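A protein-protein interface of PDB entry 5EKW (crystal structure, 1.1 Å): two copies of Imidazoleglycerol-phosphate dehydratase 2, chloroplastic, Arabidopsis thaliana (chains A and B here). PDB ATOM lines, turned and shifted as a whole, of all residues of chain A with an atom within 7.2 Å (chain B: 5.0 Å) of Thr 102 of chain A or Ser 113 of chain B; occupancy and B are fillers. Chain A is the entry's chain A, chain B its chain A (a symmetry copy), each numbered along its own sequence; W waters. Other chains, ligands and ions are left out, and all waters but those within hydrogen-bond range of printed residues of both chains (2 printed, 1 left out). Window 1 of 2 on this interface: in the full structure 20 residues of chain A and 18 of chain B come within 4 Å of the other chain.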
ATOM      1  N   ASP A 100      -8.039  13.025 -18.490  1.00  0.00           N
ATOM      2  CA  ASP A 100      -7.640  11.697 -17.960  1.00  0.00           C
ATOM      3  C   ASP A 100      -7.737  10.702 -19.115  1.00  0.00           C
ATOM      4  O   ASP A 100      -8.854  10.443 -19.560  1.00  0.00           O
ATOM      5  CB  ASP A 100      -8.583  11.310 -16.775  1.00  0.00           C
ATOM      6  CG  ASP A 100      -8.405   9.876 -16.283  1.00  0.00           C
ATOM      7  OD1 ASP A 100      -7.340   9.283 -16.572  1.00  0.00           O
ATOM      8  OD2 ASP A 100      -9.351   9.361 -15.640  1.00  0.00           O
ATOM      9  N   PHE A 101      -6.623  10.144 -19.575  1.00  0.00           N
ATOM     10  CA  PHE A 101      -6.707   9.148 -20.628  1.00  0.00           C
ATOM     11  C   PHE A 101      -5.525   8.212 -20.545  1.00  0.00           C
ATOM     12  O   PHE A 101      -4.390   8.632 -20.297  1.00  0.00           O
ATOM     13  CB  PHE A 101      -6.796   9.781 -22.023  1.00  0.00           C
ATOM     14  CG  PHE A 101      -7.409   8.840 -23.024  1.00  0.00           C
ATOM     15  CD1 PHE A 101      -8.774   8.585 -22.969  1.00  0.00           C
ATOM     16  CD2 PHE A 101      -6.640   8.134 -23.935  1.00  0.00           C
ATOM     17  CE1 PHE A 101      -9.354   7.669 -23.815  1.00  0.00           C
ATOM     18  CE2 PHE A 101      -7.225   7.210 -24.779  1.00  0.00           C
ATOM     19  CZ  PHE A 101      -8.582   6.992 -24.728  1.00  0.00           C
ATOM     20  N   THR A 102      -5.798   6.935 -20.800  1.00  0.00           N
ATOM     21  CA  THR A 102      -4.767   5.902 -20.886  1.00  0.00           C
ATOM     22  C   THR A 102      -4.799   5.301 -22.283  1.00  0.00           C
ATOM     23  O   THR A 102      -5.832   4.785 -22.704  1.00  0.00           O
ATOM     24  CB  THR A 102      -4.965   4.814 -19.816  1.00  0.00           C
ATOM     25  OG1 THR A 102      -4.905   5.421 -18.520  1.00  0.00           O
ATOM     26  CG2 THR A 102      -3.895   3.756 -19.889  1.00  0.00           C
ATOM     27  N   ALA A 103      -3.673   5.397 -22.982  1.00  0.00           N
ATOM     28  CA  ALA A 103      -3.543   4.923 -24.362  1.00  0.00           C
ATOM     29  C   ALA A 103      -2.454   3.886 -24.478  1.00  0.00           C
ATOM     30  O   ALA A 103      -1.373   4.044 -23.906  1.00  0.00           O
ATOM     31  CB  ALA A 103      -3.246   6.069 -25.308  1.00  0.00           C
ATOM     32  N   PRO A 104      -2.721   2.829 -25.262  1.00  0.00           N
ATOM     33  CA  PRO A 104      -1.664   1.912 -25.589  1.00  0.00           C
ATOM     34  C   PRO A 104      -0.993   2.239 -26.903  1.00  0.00           C
ATOM     35  O   PRO A 104      -1.525   2.973 -27.733  1.00  0.00           O
ATOM     36  CB  PRO A 104      -2.375   0.578 -25.709  1.00  0.00           C
ATOM     37  CG  PRO A 104      -3.730   0.923 -26.130  1.00  0.00           C
ATOM     38  CD  PRO A 104      -4.023   2.347 -25.752  1.00  0.00           C
ATOM     39  N   ALA A 108       2.977  -1.243 -25.015  1.00  0.00           N
ATOM     40  CA  ALA A 108       3.081  -0.085 -24.127  1.00  0.00           C
ATOM     41  C   ALA A 108       1.701   0.415 -23.725  1.00  0.00           C
ATOM     42  O   ALA A 108       0.754   0.352 -24.508  1.00  0.00           O
ATOM     43  CB  ALA A 108       3.874   1.020 -24.790  1.00  0.00           C
ATOM     44  N   LEU A 109       1.615   0.934 -22.511  1.00  0.00           N
ATOM     45  CA  LEU A 109       0.360   1.460 -21.976  1.00  0.00           C
ATOM     46  C   LEU A 109       0.698   2.593 -21.034  1.00  0.00           C
ATOM     47  O   LEU A 109       1.380   2.365 -20.037  1.00  0.00           O
ATOM     48  CB  LEU A 109      -0.423   0.360 -21.244  1.00  0.00           C
ATOM     49  CG  LEU A 109      -1.816   0.755 -20.769  1.00  0.00           C
ATOM     50  CD1 LEU A 109      -2.769   0.969 -21.941  1.00  0.00           C
ATOM     51  CD2 LEU A 109      -2.358  -0.288 -19.820  1.00  0.00           C
ATOM     52  N   ILE A 110       0.224   3.795 -21.367  1.00  0.00           N
ATOM     53  CA  ILE A 110       0.617   5.000 -20.637  1.00  0.00           C
ATOM     54  C   ILE A 110      -0.631   5.759 -20.194  1.00  0.00           C
ATOM     55  O   ILE A 110      -1.516   6.061 -21.007  1.00  0.00           O
ATOM     56  CB  ILE A 110       1.530   5.934 -21.462  1.00  0.00           C
ATOM     57  CG1 ILE A 110       2.714   5.183 -22.075  1.00  0.00           C
ATOM     58  CG2 ILE A 110       1.972   7.114 -20.611  1.00  0.00           C
ATOM     59  CD1 ILE A 110       3.718   4.597 -21.124  1.00  0.00           C
ATOM     60  N   HIS A 111      -0.685   6.046 -18.897  1.00  0.00           N
ATOM     61  CA  HIS A 111      -1.742   6.872 -18.309  1.00  0.00           C
ATOM     62  C   HIS A 111      -1.278   8.317 -18.157  1.00  0.00           C
ATOM     63  O   HIS A 111      -0.218   8.569 -17.580  1.00  0.00           O
ATOM     64  CB  HIS A 111      -2.125   6.320 -16.950  1.00  0.00           C
ATOM     65  CG  HIS A 111      -3.065   7.198 -16.206  1.00  0.00           C
ATOM     66  ND1 HIS A 111      -2.903   7.501 -14.890  1.00  0.00           N
ATOM     67  CD2 HIS A 111      -4.169   7.864 -16.614  1.00  0.00           C
ATOM     68  CE1 HIS A 111      -3.857   8.318 -14.503  1.00  0.00           C
ATOM     69  NE2 HIS A 111      -4.648   8.541 -15.532  1.00  0.00           N
ATOM     70  N   VAL A 112      -2.088   9.246 -18.673  1.00  0.00           N
ATOM     71  CA  VAL A 112      -1.892  10.668 -18.433  1.00  0.00           C
ATOM     72  C   VAL A 112      -3.128  11.264 -17.775  1.00  0.00           C
ATOM     73  O   VAL A 112      -4.240  11.119 -18.258  1.00  0.00           O
ATOM     74  CB  VAL A 112      -1.593  11.438 -19.728  1.00  0.00           C
ATOM     75  CG1 VAL A 112      -1.546  12.943 -19.460  1.00  0.00           C
ATOM     76  CG2 VAL A 112      -0.289  10.937 -20.318  1.00  0.00           C
ATOM     77  N   SER A 113      -2.893  11.959 -16.672  1.00  0.00           N
ATOM     78  CA  SER A 113      -3.901  12.751 -16.011  1.00  0.00           C
ATOM     79  C   SER A 113      -3.359  14.175 -15.869  1.00  0.00           C
ATOM     80  O   SER A 113      -2.210  14.349 -15.478  1.00  0.00           O
ATOM     81  CB  SER A 113      -4.181  12.132 -14.653  1.00  0.00           C
ATOM     82  OG  SER A 113      -5.230  12.779 -13.995  1.00  0.00           O
ATOM     83  N   ARG A 159       2.219   8.129 -16.200  1.00  0.00           N
ATOM     84  CA  ARG A 159       2.456   6.845 -15.538  1.00  0.00           C
ATOM     85  C   ARG A 159       2.603   5.726 -16.550  1.00  0.00           C
ATOM     86  O   ARG A 159       1.696   5.468 -17.354  1.00  0.00           O
ATOM     87  CB  ARG A 159       1.325   6.489 -14.574  1.00  0.00           C
ATOM     88  CG  ARG A 159       1.044   7.562 -13.544  1.00  0.00           C
ATOM     89  CD  ARG A 159       0.157   7.040 -12.432  1.00  0.00           C
ATOM     90  NE  ARG A 159      -1.113   6.549 -12.940  1.00  0.00           N
ATOM     91  CZ  ARG A 159      -1.594   5.317 -12.775  1.00  0.00           C
ATOM     92  NH1 ARG A 159      -2.776   4.989 -13.279  1.00  0.00           N
ATOM     93  NH2 ARG A 159      -0.914   4.414 -12.097  1.00  0.00           N
ATOM     94  N   LEU A 161       2.363   2.128 -17.386  1.00  0.00           N
ATOM     95  CA  LEU A 161       1.674   0.925 -16.891  1.00  0.00           C
ATOM     96  C   LEU A 161       2.216  -0.359 -17.512  1.00  0.00           C
ATOM     97  O   LEU A 161       2.092  -1.428 -16.908  1.00  0.00           O
ATOM     98  CB  LEU A 161       0.170   1.035 -17.121  1.00  0.00           C
ATOM     99  CG  LEU A 161      -0.472   2.284 -16.519  1.00  0.00           C
ATOM    100  CD1 LEU A 161      -1.963   2.301 -16.832  1.00  0.00           C
ATOM    101  CD2 LEU A 161      -0.259   2.373 -15.008  1.00  0.00           C
ATOM    102  N   ALA A 172       3.091   6.302 -27.171  1.00  0.00           N
ATOM    103  CA  ALA A 172       1.875   6.117 -26.373  1.00  0.00           C
ATOM    104  C   ALA A 172       1.708   7.281 -25.393  1.00  0.00           C
ATOM    105  O   ALA A 172       0.593   7.735 -25.141  1.00  0.00           O
ATOM    106  CB  ALA A 172       1.896   4.799 -25.643  1.00  0.00           C
ATOM    107  N   LYS A 175       0.316  10.204 -27.317  1.00  0.00           N
ATOM    108  CA  LYS A 175      -1.095   9.957 -27.638  1.00  0.00           C
ATOM    109  C   LYS A 175      -2.004  10.165 -26.432  1.00  0.00           C
ATOM    110  O   LYS A 175      -3.055  10.806 -26.540  1.00  0.00           O
ATOM    111  CB  LYS A 175      -1.260   8.543 -28.206  1.00  0.00           C
ATOM    112  CG  LYS A 175      -0.784   8.405 -29.632  1.00  0.00           C
ATOM    113  CD  LYS A 175      -0.645   6.950 -30.066  1.00  0.00           C
ATOM    114  CE  LYS A 175      -0.558   6.822 -31.575  1.00  0.00           C
ATOM    115  NZ  LYS A 175      -0.027   5.506 -31.991  1.00  0.00           N
ATOM    116  N   ALA A 176      -1.610   9.607 -25.299  1.00  0.00           N
ATOM    117  CA  ALA A 176      -2.384   9.761 -24.073  1.00  0.00           C
ATOM    118  C   ALA A 176      -2.449  11.228 -23.653  1.00  0.00           C
ATOM    119  O   ALA A 176      -3.514  11.747 -23.285  1.00  0.00           O
ATOM    120  CB  ALA A 176      -1.790   8.929 -22.948  1.00  0.00           C
ATOM    121  N   ARG A 179      -4.798  13.245 -25.915  1.00  0.00           N
ATOM    122  CA  ARG A 179      -6.217  12.994 -25.635  1.00  0.00           C
ATOM    123  C   ARG A 179      -6.631  13.611 -24.308  1.00  0.00           C
ATOM    124  O   ARG A 179      -7.731  14.166 -24.191  1.00  0.00           O
ATOM    125  CB  ARG A 179      -6.530  11.493 -25.736  1.00  0.00           C
ATOM    126  CG  ARG A 179      -6.443  11.040 -27.205  1.00  0.00           C
ATOM    127  CD  ARG A 179      -6.732   9.616 -27.648  1.00  0.00           C
ATOM    128  NE  ARG A 179      -6.821   9.618 -29.139  1.00  0.00           N
ATOM    129  CZ  ARG A 179      -7.937   9.675 -29.894  1.00  0.00           C
ATOM    130  NH1 ARG A 179      -7.836   9.743 -31.227  1.00  0.00           N
ATOM    131  NH2 ARG A 179      -9.163   9.663 -29.372  1.00  0.00           N
ATOM    132  N   ALA A 180      -5.778  13.507 -23.297  1.00  0.00           N
ATOM    133  CA  ALA A 180      -6.074  14.154 -22.009  1.00  0.00           C
ATOM    134  C   ALA A 180      -6.130  15.680 -22.143  1.00  0.00           C
ATOM    135  O   ALA A 180      -7.007  16.328 -21.578  1.00  0.00           O
ATOM    136  CB  ALA A 180      -5.056  13.736 -20.959  1.00  0.00           C
ATOM    137  N   GLY B  99     -10.267   3.510 -26.657  1.00  0.00           N
ATOM    138  CA  GLY B  99     -11.202   3.410 -25.542  1.00  0.00           C
ATOM    139  C   GLY B  99     -10.474   3.113 -24.256  1.00  0.00           C
ATOM    140  O   GLY B  99      -9.440   2.439 -24.248  1.00  0.00           O
ATOM    141  N   ASP B 100     -11.014   3.612 -23.167  1.00  0.00           N
ATOM    142  CA  ASP B 100     -10.364   3.529 -21.835  1.00  0.00           C
ATOM    143  C   ASP B 100     -11.478   3.532 -20.790  1.00  0.00           C
ATOM    144  O   ASP B 100     -12.140   4.560 -20.656  1.00  0.00           O
ATOM    145  CB  ASP B 100      -9.394   4.741 -21.659  1.00  0.00           C
ATOM    146  CG  ASP B 100      -8.825   4.881 -20.249  1.00  0.00           C
ATOM    147  OD1 ASP B 100      -8.859   3.878 -19.499  1.00  0.00           O
ATOM    148  OD2 ASP B 100      -8.379   6.004 -19.911  1.00  0.00           O
ATOM    149  N   HIS B 111      -9.601  -2.564 -15.242  1.00  0.00           N
ATOM    150  CA  HIS B 111      -9.281  -1.541 -16.240  1.00  0.00           C
ATOM    151  C   HIS B 111      -9.085  -2.172 -17.616  1.00  0.00           C
ATOM    152  O   HIS B 111      -8.306  -3.115 -17.759  1.00  0.00           O
ATOM    153  CB  HIS B 111      -8.016  -0.811 -15.836  1.00  0.00           C
ATOM    154  CG  HIS B 111      -7.520   0.122 -16.880  1.00  0.00           C
ATOM    155  ND1 HIS B 111      -6.211   0.192 -17.244  1.00  0.00           N
ATOM    156  CD2 HIS B 111      -8.177   1.010 -17.662  1.00  0.00           C
ATOM    157  CE1 HIS B 111      -6.065   1.074 -18.207  1.00  0.00           C
ATOM    158  NE2 HIS B 111      -7.246   1.596 -18.467  1.00  0.00           N
ATOM    159  N   VAL B 112      -9.794  -1.630 -18.610  1.00  0.00           N
ATOM    160  CA  VAL B 112      -9.569  -1.979 -20.005  1.00  0.00           C
ATOM    161  C   VAL B 112      -9.210  -0.735 -20.805  1.00  0.00           C
ATOM    162  O   VAL B 112      -9.913   0.263 -20.782  1.00  0.00           O
ATOM    163  CB  VAL B 112     -10.798  -2.647 -20.640  1.00  0.00           C
ATOM    164  CG1 VAL B 112     -10.579  -2.858 -22.140  1.00  0.00           C
ATOM    165  CG2 VAL B 112     -11.079  -3.956 -19.929  1.00  0.00           C
ATOM    166  N   SER B 113      -8.108  -0.838 -21.533  1.00  0.00           N
ATOM    167  CA  SER B 113      -7.704   0.156 -22.496  1.00  0.00           C
ATOM    168  C   SER B 113      -7.501  -0.548 -23.839  1.00  0.00           C
ATOM    169  O   SER B 113      -6.881  -1.606 -23.881  1.00  0.00           O
ATOM    170  CB  SER B 113      -6.416   0.797 -22.012  1.00  0.00           C
ATOM    171  OG  SER B 113      -6.019   1.852 -22.837  1.00  0.00           O
ATOM    172  N   LEU B 114      -8.016   0.036 -24.912  1.00  0.00           N
ATOM    173  CA  LEU B 114      -7.856  -0.573 -26.220  1.00  0.00           C
ATOM    174  C   LEU B 114      -7.677   0.479 -27.303  1.00  0.00           C
ATOM    175  O   LEU B 114      -8.097   1.624 -27.174  1.00  0.00           O
ATOM    176  CB  LEU B 114      -8.971  -1.573 -26.521  1.00  0.00           C
ATOM    177  CG  LEU B 114     -10.373  -1.011 -26.708  1.00  0.00           C
ATOM    178  CD1 LEU B 114     -10.643  -0.604 -28.159  1.00  0.00           C
ATOM    179  CD2 LEU B 114     -11.409  -2.043 -26.280  1.00  0.00           C
ATOM    180  N   ASP B 115      -7.019   0.044 -28.362  1.00  0.00           N
ATOM    181  CA  ASP B 115      -6.745   0.845 -29.554  1.00  0.00           C
ATOM    182  C   ASP B 115      -7.105  -0.011 -30.761  1.00  0.00           C
ATOM    183  O   ASP B 115      -6.524  -1.098 -30.954  1.00  0.00           O
ATOM    184  CB  ASP B 115      -5.245   1.222 -29.565  1.00  0.00           C
ATOM    185  CG  ASP B 115      -4.797   1.918 -30.829  1.00  0.00           C
ATOM    186  OD1 ASP B 115      -5.685   2.271 -31.618  1.00  0.00           O
ATOM    187  OD2 ASP B 115      -3.571   2.076 -31.037  1.00  0.00           O
ATOM    188  N   THR B 155      -5.425  -3.696 -30.279  1.00  0.00           N
ATOM    189  CA  THR B 155      -4.519  -3.621 -29.145  1.00  0.00           C
ATOM    190  C   THR B 155      -5.392  -3.544 -27.901  1.00  0.00           C
ATOM    191  O   THR B 155      -6.164  -2.613 -27.762  1.00  0.00           O
ATOM    192  CB  THR B 155      -3.665  -2.352 -29.216  1.00  0.00           C
ATOM    193  OG1 THR B 155      -3.014  -2.233 -30.481  1.00  0.00           O
ATOM    194  CG2 THR B 155      -2.682  -2.314 -28.086  1.00  0.00           C
ATOM    195  N   LEU B 156      -5.256  -4.508 -26.991  1.00  0.00           N
ATOM    196  CA  LEU B 156      -6.134  -4.617 -25.833  1.00  0.00           C
ATOM    197  C   LEU B 156      -5.317  -4.894 -24.578  1.00  0.00           C
ATOM    198  O   LEU B 156      -4.546  -5.848 -24.542  1.00  0.00           O
ATOM    199  CB  LEU B 156      -7.133  -5.771 -26.073  1.00  0.00           C
ATOM    200  CG  LEU B 156      -8.102  -6.106 -24.931  1.00  0.00           C
ATOM    201  CD1 LEU B 156      -8.974  -4.933 -24.524  1.00  0.00           C
ATOM    202  CD2 LEU B 156      -8.977  -7.286 -25.332  1.00  0.00           C
ATOM    203  N   HIS B 157      -5.524  -4.077 -23.550  1.00  0.00           N
ATOM    204  CA  HIS B 157      -4.929  -4.275 -22.226  1.00  0.00           C
ATOM    205  C   HIS B 157      -6.054  -4.440 -21.209  1.00  0.00           C
ATOM    206  O   HIS B 157      -6.969  -3.611 -21.138  1.00  0.00           O
ATOM    207  CB  HIS B 157      -4.053  -3.084 -21.831  1.00  0.00           C
ATOM    208  CG  HIS B 157      -2.792  -2.989 -22.612  1.00  0.00           C
ATOM    209  ND1 HIS B 157      -1.573  -3.326 -22.063  1.00  0.00           N
ATOM    210  CD2 HIS B 157      -2.561  -2.627 -23.898  1.00  0.00           C
ATOM    211  CE1 HIS B 157      -0.640  -3.153 -22.977  1.00  0.00           C
ATOM    212  NE2 HIS B 157      -1.211  -2.743 -24.100  1.00  0.00           N
HETATM  213  O   HOH W   1      -1.418   3.660 -30.377  1.00  0.00           O
HETATM  214  O   HOH W   2      -7.128   6.691 -17.624  1.00  0.00           O
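The backbone NH (N) of Thr 102 of chain A lies within hydrogen-bond range of the side-chain carboxylate (OD2) of Asp 100 of chain B (2.9 Å). O of Thr 102 of chain A is in hydrogen-bond range of OG of Ser 113 of chain B, at 2.9 Å.
N of Val 112 of chain A is in hydrogen-bond range of O of Phe 101 of chain A, 2.9 Å away. O of Leu 109 of chain A is in hydrogen-bond range of N of Leu 161 of chain A, at 2.8 Å. The side-chain carboxylate (OD1) of Asp 100 of chain B sits at hydrogen-bond distance from a ring nitrogen (NE2) of His 111 of chain B, 3.0 Å away. The backbone carbonyl oxygen (O) of Ser 113 of chain B is in hydrogen-bond range of the backbone NH (N) of His 157 of chain B. The backbone NH (N) of Asp 115 of chain B is in hydrogen-bond range of the backbone carbonyl oxygen (O) of Thr 155 of chain B (2.9 Å).
OD2 of Asp 100 of chain B touches CA of Phe 101 of chain A, 3.6 Å away. His 111 of chain B touches Thr 102 of chain A (CE1 to CG2, 3.8 Å). Pro 104 of chain A touches Ser 113 of chain B (CD to OG, 3.6 Å). CG of Pro 104 of chain A touches CB of Asp 115 of chain B (3.8 Å). Pro 104 of chain A touches Thr 155 of chain B. CB of Pro 104 of chain A touches CD2 of His 157 of chain B, at 3.7 Å. Ala 108 of chain A touches His 157 of chain B (O to NE2, 3.7 Å). CD1 of Leu 109 of chain A touches OG of Ser 113 of chain B (3.5 Å). Leu 109 of chain A touches His 157 of chain B (CD2 to CB, 3.8 Å).
Of the printed residues of chain B, Thr 102 of chain A touches Asp 100, His 111 and Ser 113. Of the printed residues of chain A, Ser 113 of chain B touches Thr 102 (2.9 Å), Pro 104 (3.6 Å) and Leu 109 (3.5 Å). Printed residues of chain B within 4 Å of Leu 109 of chain A: Ser 113 (3.5 Å) and His 157 (3.8 Å). Of the printed residues of chain A, Thr 155 of chain B touches Pro 104. Of the printed residues of chain A, His 157 of chain B touches Pro 104 (3.7 Å), Ala 108 (3.7 Å) and Leu 109 (3.8 Å). Printed residues of chain A within 4 Å of Asp 100 of chain B: Phe 101 and Thr 102. Ala 180 of chain A touches none of the printed residues of chain B. The nearest printed residue of chain B that does not touch Thr 102 of chain A is Gly 99 of chain B (4.6 Å).
Hydrophobic or aromatic side chains of chain A within 4 Å of the printed part of chain B: Phe 101, Pro 104 and Leu 109. Of the 10 printed residues of chain B, 6 touch a printed residue of chain A. Among the printed residues, 11 pairs touch across the chains. Among the printed residues, no Asp or Glu carboxylate lies within 4 Å of a Lys or Arg side-chain nitrogen of the other chain.
4 positions are printed for both chains. Of the 11 pairs that touch across the chains among the printed residues, none has its exchanged pair printed and touching as well.
Water W2 lies within hydrogen-bond range of OD2 of Asp 100 of chain B (2.7 Å), OG1 of Thr 102 of chain A (2.7 Å) and OD1 of Asp 100 of chain A (2.8 Å). Water W1 lies within hydrogen-bond range of O of Pro 104 of chain A (2.7 Å), OD2 of Asp 115 of chain B (2.8 Å) and NZ of Lys 175 of chain A (2.8 Å).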
